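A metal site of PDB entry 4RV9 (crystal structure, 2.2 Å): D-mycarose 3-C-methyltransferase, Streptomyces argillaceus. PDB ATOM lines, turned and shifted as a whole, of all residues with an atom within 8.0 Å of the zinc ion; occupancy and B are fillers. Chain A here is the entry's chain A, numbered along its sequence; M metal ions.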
ATOM      1  N   THR A  12      17.471  18.262 -31.541  1.00  0.00           N
ATOM      2  CA  THR A  12      18.682  17.618 -31.046  1.00  0.00           C
ATOM      3  C   THR A  12      19.660  18.639 -30.485  1.00  0.00           C
ATOM      4  O   THR A  12      19.632  19.826 -30.807  1.00  0.00           O
ATOM      5  CB  THR A  12      19.407  16.795 -32.120  1.00  0.00           C
ATOM      6  OG1 THR A  12      19.634  17.613 -33.283  1.00  0.00           O
ATOM      7  CG2 THR A  12      18.583  15.556 -32.508  1.00  0.00           C
ATOM      8  N   CYS A  13      20.541  18.129 -29.637  1.00  0.00           N
ATOM      9  CA  CYS A  13      21.530  18.942 -28.981  1.00  0.00           C
ATOM     10  C   CYS A  13      22.592  19.403 -29.950  1.00  0.00           C
ATOM     11  O   CYS A  13      23.168  18.624 -30.735  1.00  0.00           O
ATOM     12  CB  CYS A  13      22.166  18.216 -27.807  1.00  0.00           C
ATOM     13  SG  CYS A  13      23.590  19.079 -27.134  1.00  0.00           S
ATOM     14  N   ARG A  14      22.842  20.692 -29.854  1.00  0.00           N
ATOM     15  CA  ARG A  14      23.767  21.417 -30.685  1.00  0.00           C
ATOM     16  C   ARG A  14      25.186  20.855 -30.676  1.00  0.00           C
ATOM     17  O   ARG A  14      25.852  20.831 -31.706  1.00  0.00           O
ATOM     18  CB  ARG A  14      23.768  22.840 -30.153  1.00  0.00           C
ATOM     19  CG  ARG A  14      24.608  23.827 -30.899  1.00  0.00           C
ATOM     20  CD  ARG A  14      24.324  25.221 -30.382  1.00  0.00           C
ATOM     21  NE  ARG A  14      22.955  25.643 -30.681  1.00  0.00           N
ATOM     22  CZ  ARG A  14      21.985  25.875 -29.783  1.00  0.00           C
ATOM     23  NH1 ARG A  14      22.205  25.747 -28.481  1.00  0.00           N
ATOM     24  NH2 ARG A  14      20.787  26.248 -30.202  1.00  0.00           N
ATOM     25  N   MET A  15      25.661  20.424 -29.513  1.00  0.00           N
ATOM     26  CA  MET A  15      27.039  19.973 -29.333  1.00  0.00           C
ATOM     27  C   MET A  15      27.234  18.468 -29.540  1.00  0.00           C
ATOM     28  O   MET A  15      28.165  18.055 -30.229  1.00  0.00           O
ATOM     29  CB  MET A  15      27.518  20.329 -27.915  1.00  0.00           C
ATOM     30  CG  MET A  15      27.384  21.798 -27.558  1.00  0.00           C
ATOM     31  SD  MET A  15      28.727  22.816 -28.206  1.00  0.00           S
ATOM     32  CE  MET A  15      28.060  24.457 -27.982  1.00  0.00           C
ATOM     33  N   CYS A  16      26.377  17.654 -28.931  1.00  0.00           N
ATOM     34  CA  CYS A  16      26.585  16.188 -28.912  1.00  0.00           C
ATOM     35  C   CYS A  16      25.589  15.391 -29.747  1.00  0.00           C
ATOM     36  O   CYS A  16      25.872  14.245 -30.097  1.00  0.00           O
ATOM     37  CB  CYS A  16      26.587  15.672 -27.471  1.00  0.00           C
ATOM     38  SG  CYS A  16      24.952  15.565 -26.710  1.00  0.00           S
ATOM     39  N   GLY A  17      24.432  15.979 -30.055  1.00  0.00           N
ATOM     40  CA  GLY A  17      23.448  15.348 -30.957  1.00  0.00           C
ATOM     41  C   GLY A  17      22.318  14.574 -30.281  1.00  0.00           C
ATOM     42  O   GLY A  17      21.408  14.102 -30.950  1.00  0.00           O
ATOM     43  N   ALA A  18      22.377  14.458 -28.965  1.00  0.00           N
ATOM     44  CA  ALA A  18      21.362  13.743 -28.184  1.00  0.00           C
ATOM     45  C   ALA A  18      20.062  14.529 -28.111  1.00  0.00           C
ATOM     46  O   ALA A  18      19.955  15.635 -28.646  1.00  0.00           O
ATOM     47  CB  ALA A  18      21.882  13.448 -26.791  1.00  0.00           C
ATOM     48  N   GLN A  19      19.071  13.945 -27.451  1.00  0.00           N
ATOM     49  CA  GLN A  19      17.774  14.586 -27.254  1.00  0.00           C
ATOM     50  C   GLN A  19      17.204  14.118 -25.925  1.00  0.00           C
ATOM     51  O   GLN A  19      16.263  13.331 -25.870  1.00  0.00           O
ATOM     52  CB  GLN A  19      16.836  14.270 -28.420  1.00  0.00           C
ATOM     53  CG  GLN A  19      15.499  14.997 -28.367  1.00  0.00           C
ATOM     54  CD  GLN A  19      14.878  15.224 -29.742  1.00  0.00           C
ATOM     55  OE1 GLN A  19      15.205  14.533 -30.708  1.00  0.00           O
ATOM     56  NE2 GLN A  19      13.982  16.204 -29.834  1.00  0.00           N
ATOM     57  N   ASP A  20      17.818  14.602 -24.855  1.00  0.00           N
ATOM     58  CA  ASP A  20      17.411  14.317 -23.488  1.00  0.00           C
ATOM     59  C   ASP A  20      17.559  15.612 -22.683  1.00  0.00           C
ATOM     60  O   ASP A  20      18.584  15.855 -22.054  1.00  0.00           O
ATOM     61  CB  ASP A  20      18.263  13.175 -22.902  1.00  0.00           C
ATOM     62  CG  ASP A  20      17.809  12.734 -21.517  1.00  0.00           C
ATOM     63  OD1 ASP A  20      18.501  11.886 -20.918  1.00  0.00           O
ATOM     64  OD2 ASP A  20      16.767  13.239 -21.009  1.00  0.00           O
ATOM     65  N   TRP A  21      16.512  16.419 -22.737  1.00  0.00           N
ATOM     66  CA  TRP A  21      16.498  17.759 -22.166  1.00  0.00           C
ATOM     67  C   TRP A  21      15.767  17.843 -20.831  1.00  0.00           C
ATOM     68  O   TRP A  21      14.589  17.488 -20.749  1.00  0.00           O
ATOM     69  CB  TRP A  21      15.800  18.725 -23.117  1.00  0.00           C
ATOM     70  CG  TRP A  21      16.420  18.825 -24.463  1.00  0.00           C
ATOM     71  CD1 TRP A  21      15.941  18.285 -25.618  1.00  0.00           C
ATOM     72  CD2 TRP A  21      17.620  19.517 -24.806  1.00  0.00           C
ATOM     73  NE1 TRP A  21      16.774  18.592 -26.663  1.00  0.00           N
ATOM     74  CE2 TRP A  21      17.813  19.351 -26.193  1.00  0.00           C
ATOM     75  CE3 TRP A  21      18.560  20.258 -24.081  1.00  0.00           C
ATOM     76  CZ2 TRP A  21      18.897  19.905 -26.871  1.00  0.00           C
ATOM     77  CZ3 TRP A  21      19.644  20.812 -24.759  1.00  0.00           C
ATOM     78  CH2 TRP A  21      19.805  20.628 -26.137  1.00  0.00           C
ATOM     79  N   SER A  55      18.611  21.820 -20.285  1.00  0.00           N
ATOM     80  CA  SER A  55      19.944  21.264 -20.068  1.00  0.00           C
ATOM     81  C   SER A  55      20.045  19.853 -20.650  1.00  0.00           C
ATOM     82  O   SER A  55      19.266  18.965 -20.314  1.00  0.00           O
ATOM     83  CB  SER A  55      20.284  21.224 -18.572  1.00  0.00           C
ATOM     84  OG  SER A  55      21.550  20.611 -18.359  1.00  0.00           O
ATOM     85  N   CYS A  56      21.028  19.653 -21.527  1.00  0.00           N
ATOM     86  CA  CYS A  56      21.231  18.358 -22.162  1.00  0.00           C
ATOM     87  C   CYS A  56      21.895  17.380 -21.188  1.00  0.00           C
ATOM     88  O   CYS A  56      23.024  17.593 -20.762  1.00  0.00           O
ATOM     89  CB  CYS A  56      22.082  18.537 -23.415  1.00  0.00           C
ATOM     90  SG  CYS A  56      22.792  17.020 -24.055  1.00  0.00           S
ATOM     91  N   ARG A  57      21.197  16.294 -20.857  1.00  0.00           N
ATOM     92  CA  ARG A  57      21.722  15.300 -19.901  1.00  0.00           C
ATOM     93  C   ARG A  57      22.929  14.511 -20.416  1.00  0.00           C
ATOM     94  O   ARG A  57      23.686  13.964 -19.621  1.00  0.00           O
ATOM     95  CB  ARG A  57      20.626  14.325 -19.468  1.00  0.00           C
ATOM     96  CG  ARG A  57      19.504  14.988 -18.661  1.00  0.00           C
ATOM     97  CD  ARG A  57      18.798  13.966 -17.776  1.00  0.00           C
ATOM     98  NE  ARG A  57      17.764  14.586 -16.942  1.00  0.00           N
ATOM     99  CZ  ARG A  57      16.539  14.906 -17.360  1.00  0.00           C
ATOM    100  NH1 ARG A  57      16.152  14.676 -18.605  1.00  0.00           N
ATOM    101  NH2 ARG A  57      15.686  15.457 -16.505  1.00  0.00           N
ATOM    102  N   SER A  58      23.124  14.449 -21.730  1.00  0.00           N
ATOM    103  CA  SER A  58      24.305  13.784 -22.302  1.00  0.00           C
ATOM    104  C   SER A  58      25.602  14.566 -22.044  1.00  0.00           C
ATOM    105  O   SER A  58      26.528  14.048 -21.410  1.00  0.00           O
ATOM    106  CB  SER A  58      24.128  13.569 -23.810  1.00  0.00           C
ATOM    107  OG  SER A  58      25.344  13.146 -24.407  1.00  0.00           O
ATOM    108  N   CYS A  59      25.671  15.807 -22.534  1.00  0.00           N
ATOM    109  CA  CYS A  59      26.890  16.644 -22.445  1.00  0.00           C
ATOM    110  C   CYS A  59      26.780  17.877 -21.542  1.00  0.00           C
ATOM    111  O   CYS A  59      27.779  18.545 -21.297  1.00  0.00           O
ATOM    112  CB  CYS A  59      27.316  17.099 -23.833  1.00  0.00           C
ATOM    113  SG  CYS A  59      26.317  18.458 -24.497  1.00  0.00           S
ATOM    114  N   ARG A  60      25.557  18.179 -21.091  1.00  0.00           N
ATOM    115  CA  ARG A  60      25.279  19.328 -20.199  1.00  0.00           C
ATOM    116  C   ARG A  60      25.557  20.722 -20.793  1.00  0.00           C
ATOM    117  O   ARG A  60      25.874  21.668 -20.077  1.00  0.00           O
ATOM    118  CB  ARG A  60      25.928  19.132 -18.832  1.00  0.00           C
ATOM    119  CG  ARG A  60      25.282  18.017 -18.021  1.00  0.00           C
ATOM    120  CD  ARG A  60      23.830  18.322 -17.650  1.00  0.00           C
ATOM    121  NE  ARG A  60      23.261  17.302 -16.765  1.00  0.00           N
ATOM    122  CZ  ARG A  60      22.036  17.345 -16.244  1.00  0.00           C
ATOM    123  NH1 ARG A  60      21.220  18.371 -16.481  1.00  0.00           N
ATOM    124  NH2 ARG A  60      21.620  16.357 -15.455  1.00  0.00           N
ATOM    125  N   LEU A  61      25.398  20.831 -22.108  1.00  0.00           N
ATOM    126  CA  LEU A  61      25.140  22.122 -22.707  1.00  0.00           C
ATOM    127  C   LEU A  61      23.833  22.594 -22.124  1.00  0.00           C
ATOM    128  O   LEU A  61      22.882  21.802 -21.975  1.00  0.00           O
ATOM    129  CB  LEU A  61      25.003  22.023 -24.227  1.00  0.00           C
ATOM    130  CG  LEU A  61      24.419  23.261 -24.931  1.00  0.00           C
ATOM    131  CD1 LEU A  61      25.388  24.437 -24.879  1.00  0.00           C
ATOM    132  CD2 LEU A  61      24.036  22.949 -26.365  1.00  0.00           C
ATOM    133  N   MET A  62      23.773  23.862 -21.763  1.00  0.00           N
ATOM    134  CA  MET A  62      22.517  24.515 -21.494  1.00  0.00           C
ATOM    135  C   MET A  62      22.158  25.322 -22.747  1.00  0.00           C
ATOM    136  O   MET A  62      23.002  26.003 -23.318  1.00  0.00           O
ATOM    137  CB  MET A  62      22.620  25.387 -20.242  1.00  0.00           C
ATOM    138  CG  MET A  62      21.276  25.657 -19.595  1.00  0.00           C
ATOM    139  SD  MET A  62      21.411  26.239 -17.898  1.00  0.00           S
ATOM    140  CE  MET A  62      22.076  27.881 -18.179  1.00  0.00           C
ATOM    141  N   SER A 234      30.860  20.147 -22.668  1.00  0.00           N
ATOM    142  CA  SER A 234      30.060  20.187 -23.888  1.00  0.00           C
ATOM    143  C   SER A 234      30.896  20.500 -25.122  1.00  0.00           C
ATOM    144  O   SER A 234      30.603  20.014 -26.212  1.00  0.00           O
ATOM    145  CB  SER A 234      28.940  21.210 -23.734  1.00  0.00           C
ATOM    146  OG  SER A 234      29.460  22.496 -23.505  1.00  0.00           O
ATOM    147  N   ALA A 237      32.772  17.341 -26.092  1.00  0.00           N
ATOM    148  CA  ALA A 237      31.811  16.457 -26.776  1.00  0.00           C
ATOM    149  C   ALA A 237      31.647  16.870 -28.242  1.00  0.00           C
ATOM    150  O   ALA A 237      31.641  16.024 -29.131  1.00  0.00           O
ATOM    151  CB  ALA A 237      30.462  16.475 -26.073  1.00  0.00           C
ATOM    152  N   LEU A 238      31.528  18.170 -28.479  1.00  0.00           N
ATOM    153  CA  LEU A 238      31.386  18.696 -29.840  1.00  0.00           C
ATOM    154  C   LEU A 238      32.631  18.456 -30.679  1.00  0.00           C
ATOM    155  O   LEU A 238      32.551  17.900 -31.788  1.00  0.00           O
ATOM    156  CB  LEU A 238      31.098  20.186 -29.822  1.00  0.00           C
ATOM    157  CG  LEU A 238      31.273  20.850 -31.201  1.00  0.00           C
ATOM    158  CD1 LEU A 238      30.067  20.576 -32.089  1.00  0.00           C
ATOM    159  CD2 LEU A 238      31.547  22.339 -31.037  1.00  0.00           C
HETATM  160 ZN    ZN M   1      24.458  17.582 -25.597  1.00  0.00          ZN
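SG of Cys 13 sits close to N of Met 15, 3.4 Å away.
The backbone NH (N) of Cys 13 sits at hydrogen-bond distance from the backbone carbonyl oxygen (O) of Ala 18, at 2.7 Å.
The side-chain sulfur of Cys 59 lies close to the backbone NH of Leu 61 (3.5 Å).
SG of Cys 56 lies close to N of Ser 58 (3.5 Å).
The backbone NH (N) of Cys 56 sits at hydrogen-bond distance from the backbone carbonyl oxygen (O) of Leu 61.
The side-chain hydroxyl (OG) of Ser 58 sits close to the side-chain sulfur (SG) of Cys 16 (3.4 Å).
SG of Cys 16 lies close to N of Ala 18 (3.6 Å).
Along chain A the residues within 4 Å of the zinc ion span positions 13 to 59.
The zinc ion is bound by SG of Cys 13, SG of Cys 59, SG of Cys 56 and SG of Cys 16.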
